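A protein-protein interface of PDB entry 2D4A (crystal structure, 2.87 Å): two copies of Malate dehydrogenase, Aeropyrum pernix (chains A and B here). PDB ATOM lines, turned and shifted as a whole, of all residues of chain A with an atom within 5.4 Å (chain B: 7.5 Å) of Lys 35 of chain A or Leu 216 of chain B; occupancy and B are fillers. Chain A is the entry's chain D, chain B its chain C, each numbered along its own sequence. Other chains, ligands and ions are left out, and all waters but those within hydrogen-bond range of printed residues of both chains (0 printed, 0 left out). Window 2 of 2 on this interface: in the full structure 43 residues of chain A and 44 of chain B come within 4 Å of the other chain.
The side-chain carboxylate (OE2) of Glu 39 of chain A is in salt-bridge range of the guanidinium group (NH1) of Arg 217 of chain B (3.6 Å). OE1 of Glu 39 of chain A is in hydrogen-bond range of OH of Tyr 219 of chain B (3.0 Å). The side-chain carboxylate (OE2) of Glu 39 of chain A is in hydrogen-bond range of the side-chain hydroxyl (OH) of Tyr 223 of chain B.
The side-chain amino group (NZ) of Lys 35 of chain A lies within hydrogen-bond range of the backbone carbonyl oxygen (O) of Ala 7 of chain A (2.8 Å). OE1 of Gln 37 of chain A is in hydrogen-bond range of N of Gly 34 of chain A. NE of Arg 217 of chain B sits at hydrogen-bond distance from O of Tyr 219 of chain B (3.0 Å).
Leu 216 of chain B touches Gly 34 of chain A. N of Arg 217 of chain B touches O of Gly 34 of chain A, 3.8 Å away. N of Lys 35 of chain A touches O of Leu 216 of chain B, 3.9 Å away. Arg 217 of chain B touches Lys 35 of chain A. CG2 of Ile 213 of chain B touches O of Gly 38 of chain A, at 3.7 Å. Leu 216 of chain B touches Gly 38 of chain A (CB to CA, 3.6 Å). Ile 213 of chain B touches Leu 41 of chain A.
Lys 35 of chain A touches just these residues of chain B: Leu 216 and Arg 217. Of chain A, only Gly 34 (3.3 Å), Lys 35 (3.9 Å) and Gly 38 (3.6 Å) come within 4 Å of Leu 216 of chain B. Of the printed residues of chain B, Glu 39 of chain A touches Arg 217 (3.5 Å), Tyr 219 (3.0 Å) and Tyr 223 (2.5 Å). Of the printed residues of chain B, Gly 38 of chain A touches Ile 213 and Leu 216. Thr 214 of chain B touches none of the printed residues of chain A. Ala 30 of chain A touches none of the printed residues of chain B.
Printed residues of chain B that touch a printed residue of chain A: Ile 213, Leu 216, Arg 217, Tyr 219 and Tyr 223. Of the 14 printed residues of chain A, 5 touch a printed residue of chain B. Printed residues of chain A that touch a printed residue of chain B: Gly 34, Lys 35, Gly 38, Glu 39 and Leu 41. Hydrophobic or aromatic side chains of chain A that line the printed part of chain B: Leu 41. Along chain A the printed residues that touch a printed residue of chain B span positions 34 to 41. Among the printed residues, Asp or Glu carboxylates within 4 Å of a Lys or Arg side-chain nitrogen of the other chain: Glu 39 of chain A with Arg 217 of chain B.
No position is printed for both chains. Of the 10 pairs that touch across the chains among the printed residues, none has its exchanged pair printed and touching as well.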
ATOM      1  N   ALA A   7      19.530  -3.437  14.550  1.00  0.00           N
ATOM      2  CA  ALA A   7      18.739  -4.481  15.267  1.00  0.00           C
ATOM      3  C   ALA A   7      17.859  -3.950  16.363  1.00  0.00           C
ATOM      4  O   ALA A   7      17.228  -4.663  17.176  1.00  0.00           O
ATOM      5  CB  ALA A   7      19.642  -5.616  15.649  1.00  0.00           C
ATOM      6  N   GLY A   8      17.462  -2.623  16.444  1.00  0.00           N
ATOM      7  CA  GLY A   8      16.563  -1.959  17.356  1.00  0.00           C
ATOM      8  C   GLY A   8      15.128  -1.898  16.928  1.00  0.00           C
ATOM      9  O   GLY A   8      14.783  -2.411  15.851  1.00  0.00           O
ATOM     10  N   ALA A  30      24.324  -6.056  14.748  1.00  0.00           N
ATOM     11  CA  ALA A  30      24.186  -5.412  16.045  1.00  0.00           C
ATOM     12  C   ALA A  30      25.155  -6.076  17.020  1.00  0.00           C
ATOM     13  O   ALA A  30      25.513  -7.243  16.861  1.00  0.00           O
ATOM     14  CB  ALA A  30      22.749  -5.527  16.547  1.00  0.00           C
ATOM     15  N   THR A  32      24.779  -6.797  20.376  1.00  0.00           N
ATOM     16  CA  THR A  32      24.202  -7.822  21.242  1.00  0.00           C
ATOM     17  C   THR A  32      24.161  -9.180  20.549  1.00  0.00           C
ATOM     18  O   THR A  32      23.606  -9.318  19.460  1.00  0.00           O
ATOM     19  CB  THR A  32      22.778  -7.434  21.667  1.00  0.00           C
ATOM     20  OG1 THR A  32      22.812  -6.170  22.342  1.00  0.00           O
ATOM     21  CG2 THR A  32      22.198  -8.484  22.587  1.00  0.00           C
ATOM     22  N   PRO A  33      24.908 -10.165  21.172  1.00  0.00           N
ATOM     23  CA  PRO A  33      24.920 -11.519  20.617  1.00  0.00           C
ATOM     24  C   PRO A  33      23.560 -12.221  20.607  1.00  0.00           C
ATOM     25  O   PRO A  33      22.813 -12.167  21.585  1.00  0.00           O
ATOM     26  CB  PRO A  33      25.960 -12.235  21.477  1.00  0.00           C
ATOM     27  CG  PRO A  33      25.849 -11.545  22.791  1.00  0.00           C
ATOM     28  CD  PRO A  33      25.706 -10.090  22.408  1.00  0.00           C
ATOM     29  N   GLY A  34      23.251 -12.859  19.479  1.00  0.00           N
ATOM     30  CA  GLY A  34      21.995 -13.574  19.328  1.00  0.00           C
ATOM     31  C   GLY A  34      20.790 -12.723  18.973  1.00  0.00           C
ATOM     32  O   GLY A  34      19.815 -13.240  18.433  1.00  0.00           O
ATOM     33  N   LYS A  35      20.856 -11.424  19.264  1.00  0.00           N
ATOM     34  CA  LYS A  35      19.756 -10.495  18.991  1.00  0.00           C
ATOM     35  C   LYS A  35      19.456 -10.397  17.496  1.00  0.00           C
ATOM     36  O   LYS A  35      18.330 -10.643  17.065  1.00  0.00           O
ATOM     37  CB  LYS A  35      20.101  -9.108  19.544  1.00  0.00           C
ATOM     38  CG  LYS A  35      18.916  -8.248  19.972  1.00  0.00           C
ATOM     39  CD  LYS A  35      17.956  -7.954  18.838  1.00  0.00           C
ATOM     40  CE  LYS A  35      16.732  -7.174  19.325  1.00  0.00           C
ATOM     41  NZ  LYS A  35      17.078  -5.776  19.695  1.00  0.00           N
ATOM     42  N   PRO A  36      20.463 -10.036  16.682  1.00  0.00           N
ATOM     43  CA  PRO A  36      20.237  -9.923  15.237  1.00  0.00           C
ATOM     44  C   PRO A  36      19.903 -11.246  14.528  1.00  0.00           C
ATOM     45  O   PRO A  36      19.118 -11.267  13.582  1.00  0.00           O
ATOM     46  CB  PRO A  36      21.530  -9.263  14.737  1.00  0.00           C
ATOM     47  CG  PRO A  36      22.552  -9.742  15.701  1.00  0.00           C
ATOM     48  CD  PRO A  36      21.848  -9.668  17.030  1.00  0.00           C
ATOM     49  N   GLN A  37      20.489 -12.343  14.991  1.00  0.00           N
ATOM     50  CA  GLN A  37      20.214 -13.642  14.395  1.00  0.00           C
ATOM     51  C   GLN A  37      18.780 -14.070  14.769  1.00  0.00           C
ATOM     52  O   GLN A  37      18.044 -14.607  13.943  1.00  0.00           O
ATOM     53  CB  GLN A  37      21.258 -14.672  14.876  1.00  0.00           C
ATOM     54  CG  GLN A  37      22.714 -14.331  14.463  1.00  0.00           C
ATOM     55  CD  GLN A  37      23.555 -13.710  15.578  1.00  0.00           C
ATOM     56  OE1 GLN A  37      23.055 -12.970  16.422  1.00  0.00           O
ATOM     57  NE2 GLN A  37      24.848 -13.998  15.565  1.00  0.00           N
ATOM     58  N   GLY A  38      18.379 -13.807  16.009  1.00  0.00           N
ATOM     59  CA  GLY A  38      17.039 -14.166  16.434  1.00  0.00           C
ATOM     60  C   GLY A  38      16.011 -13.433  15.597  1.00  0.00           C
ATOM     61  O   GLY A  38      15.019 -14.005  15.134  1.00  0.00           O
ATOM     62  N   GLU A  39      16.320 -12.315  15.285  1.00  0.00           N
ATOM     63  CA  GLU A  39      15.367 -11.532  14.520  1.00  0.00           C
ATOM     64  C   GLU A  39      15.394 -11.821  13.021  1.00  0.00           C
ATOM     65  O   GLU A  39      14.350 -12.010  12.404  1.00  0.00           O
ATOM     66  CB  GLU A  39      15.611 -10.046  14.755  1.00  0.00           C
ATOM     67  CG  GLU A  39      15.209  -9.644  16.141  1.00  0.00           C
ATOM     68  CD  GLU A  39      14.272  -8.474  16.143  1.00  0.00           C
ATOM     69  OE1 GLU A  39      14.215  -7.766  17.165  1.00  0.00           O
ATOM     70  OE2 GLU A  39      13.583  -8.275  15.126  1.00  0.00           O
ATOM     71  N   ALA A  40      16.515 -11.811  12.517  1.00  0.00           N
ATOM     72  CA  ALA A  40      16.586 -12.148  11.107  1.00  0.00           C
ATOM     73  C   ALA A  40      15.857 -13.465  10.869  1.00  0.00           C
ATOM     74  O   ALA A  40      15.234 -13.668   9.819  1.00  0.00           O
ATOM     75  CB  ALA A  40      18.039 -12.261  10.669  1.00  0.00           C
ATOM     76  N   LEU A  41      15.931 -14.360  11.851  1.00  0.00           N
ATOM     77  CA  LEU A  41      15.281 -15.659  11.741  1.00  0.00           C
ATOM     78  C   LEU A  41      13.754 -15.524  11.689  1.00  0.00           C
ATOM     79  O   LEU A  41      13.115 -16.086  10.801  1.00  0.00           O
ATOM     80  CB  LEU A  41      15.698 -16.569  12.905  1.00  0.00           C
ATOM     81  CG  LEU A  41      15.357 -18.058  12.744  1.00  0.00           C
ATOM     82  CD1 LEU A  41      16.093 -18.597  11.536  1.00  0.00           C
ATOM     83  CD2 LEU A  41      15.754 -18.846  14.004  1.00  0.00           C
ATOM     84  N   ASN A  60      26.951 -10.578  14.332  1.00  0.00           N
ATOM     85  CA  ASN A  60      27.557  -9.748  15.374  1.00  0.00           C
ATOM     86  C   ASN A  60      28.921  -9.316  14.895  1.00  0.00           C
ATOM     87  O   ASN A  60      29.663  -8.635  15.602  1.00  0.00           O
ATOM     88  CB  ASN A  60      27.740 -10.527  16.667  1.00  0.00           C
ATOM     89  CG  ASN A  60      26.442 -10.859  17.322  1.00  0.00           C
ATOM     90  OD1 ASN A  60      25.594  -9.993  17.517  1.00  0.00           O
ATOM     91  ND2 ASN A  60      26.270 -12.118  17.680  1.00  0.00           N
ATOM     92  N   GLY B 210      10.123 -21.596  17.096  1.00  0.00           N
ATOM     93  CA  GLY B 210       9.588 -20.543  17.941  1.00  0.00           C
ATOM     94  C   GLY B 210      10.329 -20.289  19.242  1.00  0.00           C
ATOM     95  O   GLY B 210      10.517 -19.132  19.631  1.00  0.00           O
ATOM     96  N   ALA B 211      10.731 -21.364  19.919  1.00  0.00           N
ATOM     97  CA  ALA B 211      11.454 -21.284  21.194  1.00  0.00           C
ATOM     98  C   ALA B 211      12.859 -20.749  20.972  1.00  0.00           C
ATOM     99  O   ALA B 211      13.399 -19.992  21.788  1.00  0.00           O
ATOM    100  CB  ALA B 211      11.527 -22.665  21.833  1.00  0.00           C
ATOM    101  N   LYS B 212      13.444 -21.175  19.797  1.00  0.00           N
ATOM    102  CA  LYS B 212      14.791 -20.732  19.495  1.00  0.00           C
ATOM    103  C   LYS B 212      14.951 -19.233  19.426  1.00  0.00           C
ATOM    104  O   LYS B 212      15.970 -18.656  19.857  1.00  0.00           O
ATOM    105  CB  LYS B 212      15.273 -21.411  18.208  1.00  0.00           C
ATOM    106  CG  LYS B 212      16.691 -21.115  17.785  1.00  0.00           C
ATOM    107  CD  LYS B 212      17.218 -22.091  16.762  1.00  0.00           C
ATOM    108  CE  LYS B 212      18.638 -21.816  16.339  1.00  0.00           C
ATOM    109  NZ  LYS B 212      19.573 -21.506  17.440  1.00  0.00           N
ATOM    110  N   ILE B 213      13.968 -18.558  18.858  1.00  0.00           N
ATOM    111  CA  ILE B 213      14.066 -17.099  18.694  1.00  0.00           C
ATOM    112  C   ILE B 213      13.944 -16.351  19.997  1.00  0.00           C
ATOM    113  O   ILE B 213      14.304 -15.195  20.161  1.00  0.00           O
ATOM    114  CB  ILE B 213      13.146 -16.556  17.611  1.00  0.00           C
ATOM    115  CG1 ILE B 213      11.663 -16.788  17.936  1.00  0.00           C
ATOM    116  CG2 ILE B 213      13.437 -17.154  16.232  1.00  0.00           C
ATOM    117  CD1 ILE B 213      10.721 -16.262  16.878  1.00  0.00           C
ATOM    118  N   THR B 214      13.018 -17.021  20.635  1.00  0.00           N
ATOM    119  CA  THR B 214      12.849 -16.400  21.945  1.00  0.00           C
ATOM    120  C   THR B 214      14.210 -16.462  22.633  1.00  0.00           C
ATOM    121  O   THR B 214      14.717 -15.458  23.124  1.00  0.00           O
ATOM    122  CB  THR B 214      11.831 -17.171  22.798  1.00  0.00           C
ATOM    123  OG1 THR B 214      10.592 -17.269  22.086  1.00  0.00           O
ATOM    124  CG2 THR B 214      11.599 -16.461  24.111  1.00  0.00           C
ATOM    125  N   GLU B 215      14.785 -17.662  22.648  1.00  0.00           N
ATOM    126  CA  GLU B 215      16.092 -17.934  23.237  1.00  0.00           C
ATOM    127  C   GLU B 215      17.106 -16.884  22.754  1.00  0.00           C
ATOM    128  O   GLU B 215      17.813 -16.278  23.556  1.00  0.00           O
ATOM    129  CB  GLU B 215      16.522 -19.359  22.827  1.00  0.00           C
ATOM    130  CG  GLU B 215      17.922 -19.844  23.255  1.00  0.00           C
ATOM    131  CD  GLU B 215      18.457 -20.989  22.365  1.00  0.00           C
ATOM    132  OE1 GLU B 215      17.823 -22.072  22.318  1.00  0.00           O
ATOM    133  OE2 GLU B 215      19.513 -20.796  21.713  1.00  0.00           O
ATOM    134  N   LEU B 216      17.139 -16.650  21.443  1.00  0.00           N
ATOM    135  CA  LEU B 216      18.065 -15.694  20.823  1.00  0.00           C
ATOM    136  C   LEU B 216      17.813 -14.198  21.062  1.00  0.00           C
ATOM    137  O   LEU B 216      18.605 -13.533  21.723  1.00  0.00           O
ATOM    138  CB  LEU B 216      18.143 -15.950  19.307  1.00  0.00           C
ATOM    139  CG  LEU B 216      18.863 -17.233  18.867  1.00  0.00           C
ATOM    140  CD1 LEU B 216      18.928 -17.333  17.345  1.00  0.00           C
ATOM    141  CD2 LEU B 216      20.259 -17.234  19.445  1.00  0.00           C
ATOM    142  N   ARG B 217      16.721 -13.669  20.522  1.00  0.00           N
ATOM    143  CA  ARG B 217      16.424 -12.248  20.667  1.00  0.00           C
ATOM    144  C   ARG B 217      15.772 -11.818  21.987  1.00  0.00           C
ATOM    145  O   ARG B 217      15.753 -10.632  22.304  1.00  0.00           O
ATOM    146  CB  ARG B 217      15.561 -11.771  19.490  1.00  0.00           C
ATOM    147  CG  ARG B 217      14.184 -12.426  19.393  1.00  0.00           C
ATOM    148  CD  ARG B 217      13.397 -11.813  18.256  1.00  0.00           C
ATOM    149  NE  ARG B 217      11.961 -12.071  18.340  1.00  0.00           N
ATOM    150  CZ  ARG B 217      11.084 -11.623  17.447  1.00  0.00           C
ATOM    151  NH1 ARG B 217      11.504 -10.906  16.413  1.00  0.00           N
ATOM    152  NH2 ARG B 217       9.793 -11.882  17.584  1.00  0.00           N
ATOM    153  N   GLY B 218      15.222 -12.760  22.746  1.00  0.00           N
ATOM    154  CA  GLY B 218      14.619 -12.393  24.012  1.00  0.00           C
ATOM    155  C   GLY B 218      13.103 -12.363  24.094  1.00  0.00           C
ATOM    156  O   GLY B 218      12.555 -12.247  25.189  1.00  0.00           O
ATOM    157  N   TYR B 219      12.412 -12.446  22.963  1.00  0.00           N
ATOM    158  CA  TYR B 219      10.954 -12.444  22.998  1.00  0.00           C
ATOM    159  C   TYR B 219      10.333 -13.270  21.877  1.00  0.00           C
ATOM    160  O   TYR B 219      10.880 -13.358  20.781  1.00  0.00           O
ATOM    161  CB  TYR B 219      10.412 -11.017  22.958  1.00  0.00           C
ATOM    162  CG  TYR B 219      10.696 -10.263  21.686  1.00  0.00           C
ATOM    163  CD1 TYR B 219      11.976  -9.782  21.406  1.00  0.00           C
ATOM    164  CD2 TYR B 219       9.668  -9.987  20.778  1.00  0.00           C
ATOM    165  CE1 TYR B 219      12.220  -9.038  20.258  1.00  0.00           C
ATOM    166  CE2 TYR B 219       9.902  -9.246  19.628  1.00  0.00           C
ATOM    167  CZ  TYR B 219      11.176  -8.773  19.378  1.00  0.00           C
ATOM    168  OH  TYR B 219      11.400  -8.009  18.263  1.00  0.00           O
ATOM    169  N   TYR B 223       6.901 -11.389  13.651  1.00  0.00           N
ATOM    170  CA  TYR B 223       6.865 -11.154  12.211  1.00  0.00           C
ATOM    171  C   TYR B 223       6.153 -12.338  11.550  1.00  0.00           C
ATOM    172  O   TYR B 223       5.319 -12.150  10.666  1.00  0.00           O
ATOM    173  CB  TYR B 223       8.279 -10.992  11.633  1.00  0.00           C
ATOM    174  CG  TYR B 223       9.131  -9.937  12.314  1.00  0.00           C
ATOM    175  CD1 TYR B 223      10.464 -10.208  12.631  1.00  0.00           C
ATOM    176  CD2 TYR B 223       8.595  -8.699  12.692  1.00  0.00           C
ATOM    177  CE1 TYR B 223      11.245  -9.291  13.317  1.00  0.00           C
ATOM    178  CE2 TYR B 223       9.373  -7.761  13.383  1.00  0.00           C
ATOM    179  CZ  TYR B 223      10.701  -8.073  13.698  1.00  0.00           C
ATOM    180  OH  TYR B 223      11.486  -7.211  14.436  1.00  0.00           O
